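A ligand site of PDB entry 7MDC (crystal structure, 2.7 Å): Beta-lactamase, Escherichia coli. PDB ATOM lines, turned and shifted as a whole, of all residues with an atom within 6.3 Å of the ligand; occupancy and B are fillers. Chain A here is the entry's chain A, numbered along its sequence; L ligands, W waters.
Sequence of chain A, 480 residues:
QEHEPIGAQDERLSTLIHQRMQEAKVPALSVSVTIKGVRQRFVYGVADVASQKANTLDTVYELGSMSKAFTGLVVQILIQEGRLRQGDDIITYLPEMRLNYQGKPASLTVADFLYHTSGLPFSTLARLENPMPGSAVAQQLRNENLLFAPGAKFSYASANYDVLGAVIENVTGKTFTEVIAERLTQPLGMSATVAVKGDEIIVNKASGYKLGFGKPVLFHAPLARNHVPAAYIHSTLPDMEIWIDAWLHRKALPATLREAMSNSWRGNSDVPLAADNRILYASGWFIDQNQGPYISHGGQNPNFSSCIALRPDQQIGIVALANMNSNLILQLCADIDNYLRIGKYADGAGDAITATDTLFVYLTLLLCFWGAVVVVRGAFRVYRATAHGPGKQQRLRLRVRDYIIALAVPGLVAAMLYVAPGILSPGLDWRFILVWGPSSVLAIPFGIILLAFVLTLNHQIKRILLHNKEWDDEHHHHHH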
ATOM      1  N   LEU A  63      10.222 -36.888 -19.909  1.00  0.00           N
ATOM      2  CA  LEU A  63      10.387 -37.145 -21.340  1.00  0.00           C
ATOM      3  C   LEU A  63      10.187 -35.904 -22.222  1.00  0.00           C
ATOM      4  O   LEU A  63      10.491 -35.960 -23.423  1.00  0.00           O
ATOM      5  CB  LEU A  63       9.436 -38.253 -21.783  1.00  0.00           C
ATOM      6  CG  LEU A  63       9.671 -39.661 -21.247  1.00  0.00           C
ATOM      7  CD1 LEU A  63       8.770 -40.669 -21.954  1.00  0.00           C
ATOM      8  CD2 LEU A  63      11.113 -40.022 -21.430  1.00  0.00           C
ATOM      9  N   GLY A  64       9.714 -34.795 -21.671  1.00  0.00           N
ATOM     10  CA  GLY A  64       9.497 -33.654 -22.533  1.00  0.00           C
ATOM     11  C   GLY A  64       8.464 -33.994 -23.588  1.00  0.00           C
ATOM     12  O   GLY A  64       7.494 -34.724 -23.339  1.00  0.00           O
ATOM     13  N   SER A  65       8.679 -33.473 -24.802  1.00  0.00           N
ATOM     14  CA  SER A  65       7.735 -33.723 -25.879  1.00  0.00           C
ATOM     15  C   SER A  65       7.735 -35.168 -26.357  1.00  0.00           C
ATOM     16  O   SER A  65       6.911 -35.514 -27.198  1.00  0.00           O
ATOM     17  CB  SER A  65       8.025 -32.803 -27.053  1.00  0.00           C
ATOM     18  OG  SER A  65       7.659 -31.464 -26.735  1.00  0.00           O
ATOM     19  N   MET A  66       8.620 -36.028 -25.838  1.00  0.00           N
ATOM     20  CA  MET A  66       8.445 -37.433 -26.165  1.00  0.00           C
ATOM     21  C   MET A  66       7.302 -38.070 -25.373  1.00  0.00           C
ATOM     22  O   MET A  66       7.003 -39.259 -25.582  1.00  0.00           O
ATOM     23  CB  MET A  66       9.751 -38.175 -25.965  1.00  0.00           C
ATOM     24  CG  MET A  66      10.924 -37.480 -26.614  1.00  0.00           C
ATOM     25  SD  MET A  66      12.602 -38.046 -26.214  1.00  0.00           S
ATOM     26  CE  MET A  66      12.364 -39.781 -25.846  1.00  0.00           C
ATOM     27  N   LYS A  68       4.394 -36.967 -26.045  1.00  0.00           N
ATOM     28  CA  LYS A  68       3.293 -36.846 -26.992  1.00  0.00           C
ATOM     29  C   LYS A  68       3.061 -38.140 -27.773  1.00  0.00           C
ATOM     30  O   LYS A  68       1.947 -38.373 -28.253  1.00  0.00           O
ATOM     31  CB  LYS A  68       3.547 -35.690 -27.953  1.00  0.00           C
ATOM     32  CG  LYS A  68       3.571 -34.336 -27.267  1.00  0.00           C
ATOM     33  CD  LYS A  68       4.014 -33.247 -28.200  1.00  0.00           C
ATOM     34  CE  LYS A  68       3.783 -31.884 -27.596  1.00  0.00           C
ATOM     35  NZ  LYS A  68       4.666 -31.653 -26.429  1.00  0.00           N
ATOM     36  N   PHE A 122       1.421 -19.244 -29.631  1.00  0.00           N
ATOM     37  CA  PHE A 122       2.559 -19.755 -28.868  1.00  0.00           C
ATOM     38  C   PHE A 122       2.335 -19.667 -27.368  1.00  0.00           C
ATOM     39  O   PHE A 122       2.831 -20.515 -26.619  1.00  0.00           O
ATOM     40  CB  PHE A 122       3.849 -18.998 -29.207  1.00  0.00           C
ATOM     41  CG  PHE A 122       5.048 -19.490 -28.445  1.00  0.00           C
ATOM     42  CD1 PHE A 122       5.561 -20.753 -28.696  1.00  0.00           C
ATOM     43  CD2 PHE A 122       5.642 -18.720 -27.449  1.00  0.00           C
ATOM     44  CE1 PHE A 122       6.645 -21.233 -27.989  1.00  0.00           C
ATOM     45  CE2 PHE A 122       6.742 -19.192 -26.740  1.00  0.00           C
ATOM     46  CZ  PHE A 122       7.239 -20.447 -27.000  1.00  0.00           C
ATOM     47  N   LEU A 125       1.415 -22.366 -24.363  1.00  0.00           N
ATOM     48  CA  LEU A 125       2.384 -23.124 -23.571  1.00  0.00           C
ATOM     49  C   LEU A 125       2.599 -22.477 -22.200  1.00  0.00           C
ATOM     50  O   LEU A 125       2.625 -23.171 -21.184  1.00  0.00           O
ATOM     51  CB  LEU A 125       3.715 -23.243 -24.321  1.00  0.00           C
ATOM     52  CG  LEU A 125       4.920 -23.810 -23.552  1.00  0.00           C
ATOM     53  CD1 LEU A 125       4.799 -25.304 -23.355  1.00  0.00           C
ATOM     54  CD2 LEU A 125       6.262 -23.459 -24.211  1.00  0.00           C
ATOM     55  N   GLU A 129       1.440 -24.748 -18.953  1.00  0.00           N
ATOM     56  CA  GLU A 129       2.533 -25.193 -18.113  1.00  0.00           C
ATOM     57  C   GLU A 129       2.468 -24.602 -16.710  1.00  0.00           C
ATOM     58  O   GLU A 129       3.193 -25.087 -15.820  1.00  0.00           O
ATOM     59  CB  GLU A 129       3.880 -24.824 -18.763  1.00  0.00           C
ATOM     60  CG  GLU A 129       4.310 -23.389 -18.496  1.00  0.00           C
ATOM     61  CD  GLU A 129       5.677 -23.051 -19.052  1.00  0.00           C
ATOM     62  OE1 GLU A 129       6.299 -23.897 -19.744  1.00  0.00           O
ATOM     63  OE2 GLU A 129       6.136 -21.926 -18.784  1.00  0.00           O
ATOM     64  N   TYR A 156       3.839 -26.083 -34.737  1.00  0.00           N
ATOM     65  CA  TYR A 156       3.931 -26.889 -33.516  1.00  0.00           C
ATOM     66  C   TYR A 156       3.592 -26.066 -32.279  1.00  0.00           C
ATOM     67  O   TYR A 156       4.207 -25.013 -32.022  1.00  0.00           O
ATOM     68  CB  TYR A 156       5.330 -27.492 -33.409  1.00  0.00           C
ATOM     69  CG  TYR A 156       5.567 -28.459 -32.247  1.00  0.00           C
ATOM     70  CD1 TYR A 156       5.893 -28.003 -30.970  1.00  0.00           C
ATOM     71  CD2 TYR A 156       5.508 -29.832 -32.452  1.00  0.00           C
ATOM     72  CE1 TYR A 156       6.126 -28.879 -29.937  1.00  0.00           C
ATOM     73  CE2 TYR A 156       5.747 -30.720 -31.419  1.00  0.00           C
ATOM     74  CZ  TYR A 156       6.054 -30.248 -30.163  1.00  0.00           C
ATOM     75  OH  TYR A 156       6.307 -31.154 -29.149  1.00  0.00           O
ATOM     76  N   SER A 158       2.950 -27.039 -28.118  1.00  0.00           N
ATOM     77  CA  SER A 158       2.984 -28.121 -27.141  1.00  0.00           C
ATOM     78  C   SER A 158       1.581 -28.428 -26.603  1.00  0.00           C
ATOM     79  O   SER A 158       1.271 -29.602 -26.341  1.00  0.00           O
ATOM     80  CB  SER A 158       3.926 -27.742 -26.000  1.00  0.00           C
ATOM     81  OG  SER A 158       4.349 -28.889 -25.283  1.00  0.00           O
ATOM     82  N   ALA A 159       0.726 -27.407 -26.487  1.00  0.00           N
ATOM     83  CA  ALA A 159      -0.552 -27.509 -25.806  1.00  0.00           C
ATOM     84  C   ALA A 159      -1.569 -28.351 -26.572  1.00  0.00           C
ATOM     85  O   ALA A 159      -2.554 -28.783 -25.971  1.00  0.00           O
ATOM     86  CB  ALA A 159      -1.120 -26.116 -25.529  1.00  0.00           C
ATOM     87  N   HIS A 227      -0.612 -30.303 -18.159  1.00  0.00           N
ATOM     88  CA  HIS A 227       0.445 -30.298 -19.161  1.00  0.00           C
ATOM     89  C   HIS A 227       1.183 -31.629 -19.267  1.00  0.00           C
ATOM     90  O   HIS A 227       2.125 -31.743 -20.045  1.00  0.00           O
ATOM     91  CB  HIS A 227       1.443 -29.193 -18.850  1.00  0.00           C
ATOM     92  CG  HIS A 227       2.276 -28.790 -20.032  1.00  0.00           C
ATOM     93  ND1 HIS A 227       1.784 -28.757 -21.315  1.00  0.00           N
ATOM     94  CD2 HIS A 227       3.567 -28.388 -20.111  1.00  0.00           C
ATOM     95  CE1 HIS A 227       2.727 -28.356 -22.147  1.00  0.00           C
ATOM     96  NE2 HIS A 227       3.819 -28.119 -21.440  1.00  0.00           N
ATOM     97  N   ALA A 230       1.610 -33.549 -22.690  1.00  0.00           N
ATOM     98  CA  ALA A 230       2.557 -32.947 -23.623  1.00  0.00           C
ATOM     99  C   ALA A 230       4.017 -33.014 -23.175  1.00  0.00           C
ATOM    100  O   ALA A 230       4.904 -33.073 -24.028  1.00  0.00           O
ATOM    101  CB  ALA A 230       2.215 -31.479 -23.861  1.00  0.00           C
ATOM    102  N   ALA A 231       4.299 -33.028 -21.861  1.00  0.00           N
ATOM    103  CA  ALA A 231       5.647 -32.720 -21.429  1.00  0.00           C
ATOM    104  C   ALA A 231       6.176 -33.519 -20.231  1.00  0.00           C
ATOM    105  O   ALA A 231       7.381 -33.469 -19.984  1.00  0.00           O
ATOM    106  CB  ALA A 231       5.744 -31.233 -21.083  1.00  0.00           C
ATOM    107  N   TYR A 232       5.338 -34.235 -19.471  1.00  0.00           N
ATOM    108  CA  TYR A 232       5.757 -34.713 -18.163  1.00  0.00           C
ATOM    109  C   TYR A 232       5.412 -36.186 -17.932  1.00  0.00           C
ATOM    110  O   TYR A 232       5.135 -36.578 -16.800  1.00  0.00           O
ATOM    111  CB  TYR A 232       5.166 -33.857 -17.036  1.00  0.00           C
ATOM    112  CG  TYR A 232       5.521 -32.397 -17.136  1.00  0.00           C
ATOM    113  CD1 TYR A 232       6.836 -31.994 -17.005  1.00  0.00           C
ATOM    114  CD2 TYR A 232       4.545 -31.424 -17.354  1.00  0.00           C
ATOM    115  CE1 TYR A 232       7.184 -30.652 -17.097  1.00  0.00           C
ATOM    116  CE2 TYR A 232       4.871 -30.076 -17.447  1.00  0.00           C
ATOM    117  CZ  TYR A 232       6.203 -29.696 -17.324  1.00  0.00           C
ATOM    118  OH  TYR A 232       6.585 -28.378 -17.411  1.00  0.00           O
ATOM    119  N   HIS A 297      11.585 -37.667 -32.556  1.00  0.00           N
ATOM    120  CA  HIS A 297      11.036 -36.576 -31.772  1.00  0.00           C
ATOM    121  C   HIS A 297      12.026 -36.231 -30.657  1.00  0.00           C
ATOM    122  O   HIS A 297      12.656 -37.129 -30.107  1.00  0.00           O
ATOM    123  CB  HIS A 297       9.671 -36.922 -31.180  1.00  0.00           C
ATOM    124  CG  HIS A 297       8.766 -35.738 -31.036  1.00  0.00           C
ATOM    125  ND1 HIS A 297       9.060 -34.670 -30.231  1.00  0.00           N
ATOM    126  CD2 HIS A 297       7.559 -35.465 -31.592  1.00  0.00           C
ATOM    127  CE1 HIS A 297       8.088 -33.773 -30.303  1.00  0.00           C
ATOM    128  NE2 HIS A 297       7.156 -34.242 -31.120  1.00  0.00           N
ATOM    129  N   GLY A 298      12.172 -34.930 -30.359  1.00  0.00           N
ATOM    130  CA  GLY A 298      12.985 -34.476 -29.250  1.00  0.00           C
ATOM    131  C   GLY A 298      12.167 -34.222 -27.980  1.00  0.00           C
ATOM    132  O   GLY A 298      10.939 -34.053 -28.008  1.00  0.00           O
ATOM    133  N   GLY A 299      12.862 -34.207 -26.853  1.00  0.00           N
ATOM    134  CA  GLY A 299      12.265 -33.838 -25.588  1.00  0.00           C
ATOM    135  C   GLY A 299      12.929 -32.598 -25.045  1.00  0.00           C
ATOM    136  O   GLY A 299      14.161 -32.520 -25.026  1.00  0.00           O
ATOM    137  N   GLN A 300      12.140 -31.613 -24.624  1.00  0.00           N
ATOM    138  CA  GLN A 300      12.715 -30.356 -24.179  1.00  0.00           C
ATOM    139  C   GLN A 300      11.806 -29.748 -23.120  1.00  0.00           C
ATOM    140  O   GLN A 300      10.771 -29.143 -23.445  1.00  0.00           O
ATOM    141  CB  GLN A 300      12.896 -29.413 -25.362  1.00  0.00           C
ATOM    142  CG  GLN A 300      13.517 -28.091 -24.978  1.00  0.00           C
ATOM    143  CD  GLN A 300      13.633 -27.144 -26.156  1.00  0.00           C
ATOM    144  OE1 GLN A 300      13.812 -27.567 -27.296  1.00  0.00           O
ATOM    145  NE2 GLN A 300      13.529 -25.841 -25.887  1.00  0.00           N
ATOM    146  N   ASN A 301      12.187 -29.904 -21.854  1.00  0.00           N
ATOM    147  CA  ASN A 301      11.554 -29.265 -20.710  1.00  0.00           C
ATOM    148  C   ASN A 301      12.505 -28.235 -20.138  1.00  0.00           C
ATOM    149  O   ASN A 301      13.635 -28.111 -20.601  1.00  0.00           O
ATOM    150  CB  ASN A 301      11.182 -30.302 -19.646  1.00  0.00           C
ATOM    151  CG  ASN A 301      10.014 -31.163 -20.069  1.00  0.00           C
ATOM    152  OD1 ASN A 301       9.325 -30.854 -21.039  1.00  0.00           O
ATOM    153  ND2 ASN A 301       9.796 -32.264 -19.346  1.00  0.00           N
ATOM    154  N   PRO A 302      12.059 -27.417 -19.173  1.00  0.00           N
ATOM    155  CA  PRO A 302      12.963 -26.391 -18.636  1.00  0.00           C
ATOM    156  C   PRO A 302      14.259 -26.941 -18.038  1.00  0.00           C
ATOM    157  O   PRO A 302      15.254 -26.226 -17.980  1.00  0.00           O
ATOM    158  CB  PRO A 302      12.106 -25.715 -17.556  1.00  0.00           C
ATOM    159  CG  PRO A 302      10.728 -25.835 -18.066  1.00  0.00           C
ATOM    160  CD  PRO A 302      10.660 -27.192 -18.746  1.00  0.00           C
ATOM    161  N   LEU A 330      19.302 -32.740 -27.799  1.00  0.00           N
ATOM    162  CA  LEU A 330      18.246 -32.761 -28.810  1.00  0.00           C
ATOM    163  C   LEU A 330      18.775 -33.242 -30.159  1.00  0.00           C
ATOM    164  O   LEU A 330      18.055 -33.914 -30.897  1.00  0.00           O
ATOM    165  CB  LEU A 330      17.634 -31.368 -28.936  1.00  0.00           C
ATOM    166  CG  LEU A 330      16.664 -30.969 -27.821  1.00  0.00           C
ATOM    167  CD1 LEU A 330      16.402 -29.469 -27.849  1.00  0.00           C
ATOM    168  CD2 LEU A 330      15.381 -31.727 -28.001  1.00  0.00           C
ATOM    169  N   PHE A 432       7.408 -16.789 -17.429  1.00  0.00           N
ATOM    170  CA  PHE A 432       7.809 -17.694 -18.494  1.00  0.00           C
ATOM    171  C   PHE A 432       9.288 -17.540 -18.820  1.00  0.00           C
ATOM    172  O   PHE A 432       9.986 -18.527 -19.079  1.00  0.00           O
ATOM    173  CB  PHE A 432       6.963 -17.434 -19.736  1.00  0.00           C
ATOM    174  CG  PHE A 432       7.245 -18.342 -20.888  1.00  0.00           C
ATOM    175  CD1 PHE A 432       6.593 -19.557 -20.992  1.00  0.00           C
ATOM    176  CD2 PHE A 432       8.137 -17.977 -21.871  1.00  0.00           C
ATOM    177  CE1 PHE A 432       6.844 -20.402 -22.071  1.00  0.00           C
ATOM    178  CE2 PHE A 432       8.399 -18.818 -22.941  1.00  0.00           C
ATOM    179  CZ  PHE A 432       7.755 -20.037 -23.041  1.00  0.00           C
ATOM    180  N   TRP A 436      12.220 -20.739 -18.456  1.00  0.00           N
ATOM    181  CA  TRP A 436      12.955 -21.328 -19.573  1.00  0.00           C
ATOM    182  C   TRP A 436      14.358 -20.785 -19.781  1.00  0.00           C
ATOM    183  O   TRP A 436      15.197 -21.496 -20.335  1.00  0.00           O
ATOM    184  CB  TRP A 436      12.169 -21.187 -20.884  1.00  0.00           C
ATOM    185  CG  TRP A 436      10.972 -22.102 -20.987  1.00  0.00           C
ATOM    186  CD1 TRP A 436       9.672 -21.797 -20.680  1.00  0.00           C
ATOM    187  CD2 TRP A 436      10.983 -23.474 -21.409  1.00  0.00           C
ATOM    188  NE1 TRP A 436       8.868 -22.898 -20.898  1.00  0.00           N
ATOM    189  CE2 TRP A 436       9.642 -23.935 -21.347  1.00  0.00           C
ATOM    190  CE3 TRP A 436      11.983 -24.363 -21.838  1.00  0.00           C
ATOM    191  CZ2 TRP A 436       9.282 -25.256 -21.693  1.00  0.00           C
ATOM    192  CZ3 TRP A 436      11.615 -25.664 -22.196  1.00  0.00           C
ATOM    193  CH2 TRP A 436      10.276 -26.102 -22.112  1.00  0.00           C
HETATM  194  C1  LIG L   1      11.116 -21.101 -24.889  1.00  0.00           C
HETATM  195  C2  LIG L   1      10.067 -22.198 -25.030  1.00  0.00           C
HETATM  196  C3  LIG L   1      10.665 -23.563 -25.378  1.00  0.00           C
HETATM  197  C4  LIG L   1       9.579 -24.543 -25.816  1.00  0.00           C
HETATM  198  C5  LIG L   1      10.106 -25.970 -25.916  1.00  0.00           C
HETATM  199  C6  LIG L   1       8.994 -26.977 -26.152  1.00  0.00           C
HETATM  200  N1  LIG L   1       8.928 -28.184 -25.351  1.00  0.00           N
HETATM  201  C7  LIG L   1       7.886 -29.185 -25.546  1.00  0.00           C
HETATM  202  C8  LIG L   1       7.590 -29.833 -24.202  1.00  0.00           C
HETATM  203  C9  LIG L   1       7.024 -28.889 -23.144  1.00  0.00           C
HETATM  204  N2  LIG L   1       7.775 -28.522 -21.967  1.00  0.00           N
HETATM  205  O1  LIG L   1       5.942 -28.436 -23.309  1.00  0.00           O
HETATM  206  O2  LIG L   1       9.816 -30.649 -26.280  1.00  0.00           O
HETATM  207  O3  LIG L   1       8.262 -29.571 -27.898  1.00  0.00           O
HETATM  208  O4  LIG L   1       8.198 -26.791 -27.009  1.00  0.00           O
HETATM  209  B1  LIG L   1       8.404 -30.241 -26.585  1.00  0.00           B
HETATM  210  O   HOH W   1       6.766 -26.761 -19.699  1.00  0.00           O
HETATM  211  O   HOH W   2      10.470 -31.321 -29.055  1.00  0.00           O
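The backbone NH of Ser 65 lies close to an oxygen (O2) of the ligand (3.4 Å). OG of Ser 65 is covalently linked to B1 of the ligand (1.4 Å). OG of Ser 158 is in hydrogen-bond range of O1 of the ligand (2.6 Å). An oxygen (O3) of the ligand is in hydrogen-bond range of the side-chain hydroxyl of Tyr 156. The backbone NH (N) of Gln 300 is in hydrogen-bond range of an oxygen (O2) of the ligand. The backbone carbonyl oxygen (O) of Gln 300 sits at hydrogen-bond distance from a nitrogen (N1) of the ligand (2.8 Å). O1 of the ligand sits at hydrogen-bond distance from NE2 of His 227 (2.8 Å). OD1 of Asn 301 lies within hydrogen-bond range of N2 of the ligand (2.9 Å).
NZ of Lys 68 lies within hydrogen-bond range of OG of Ser 65, 3.0 Å away. NZ of Lys 68 lies within hydrogen-bond range of OG of Ser 158 (3.0 Å). OH of Tyr 156 sits close to NZ of Lys 68 (3.2 Å). O of Ala 231 is in hydrogen-bond range of ND2 of Asn 301 (2.8 Å). The side-chain amide nitrogen (ND2) of Asn 301 lies close to the backbone NH (N) of Gly 64 (3.4 Å). O of Ala 231 sits at hydrogen-bond distance from N of Gly 64 (3.2 Å). OE1 of Glu 129 is in hydrogen-bond range of NE1 of Trp 436 (3.0 Å). The backbone carbonyl oxygen of Ala 230 lies within hydrogen-bond range of the side-chain amino group of Lys 68 (2.8 Å).
NZ of Lys 68 touches B1 of the ligand, 3.999 Å away. Phe 122 touches the ligand. Leu 125 touches the ligand (CD1 to O1, 3.3 Å). CB of Ala 231 touches C9 of the ligand, at 3.4 Å. Gly 298 touches the ligand. Gly 299 touches the ligand. Phe 432 touches the ligand (CZ to C2, 3.7 Å). Trp 436 touches the ligand (CH2 to N2, 3.5 Å). Hydrophobic or aromatic side chains that line the ligand: Phe 122, Leu 125, Tyr 156, His 227, Ala 231, Phe 432 and Trp 436. Of the 24 residues printed, 14 come within 4 Å of the ligand.
Water W2 lies within hydrogen-bond range of O2 of the ligand (2.9 Å) and O of Gly 298 (3.0 Å). Water W1 lies within hydrogen-bond range of OH of Tyr 232 (2.8 Å), OE1 of Glu 129 (2.9 Å) and N2 of the ligand (3.0 Å).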
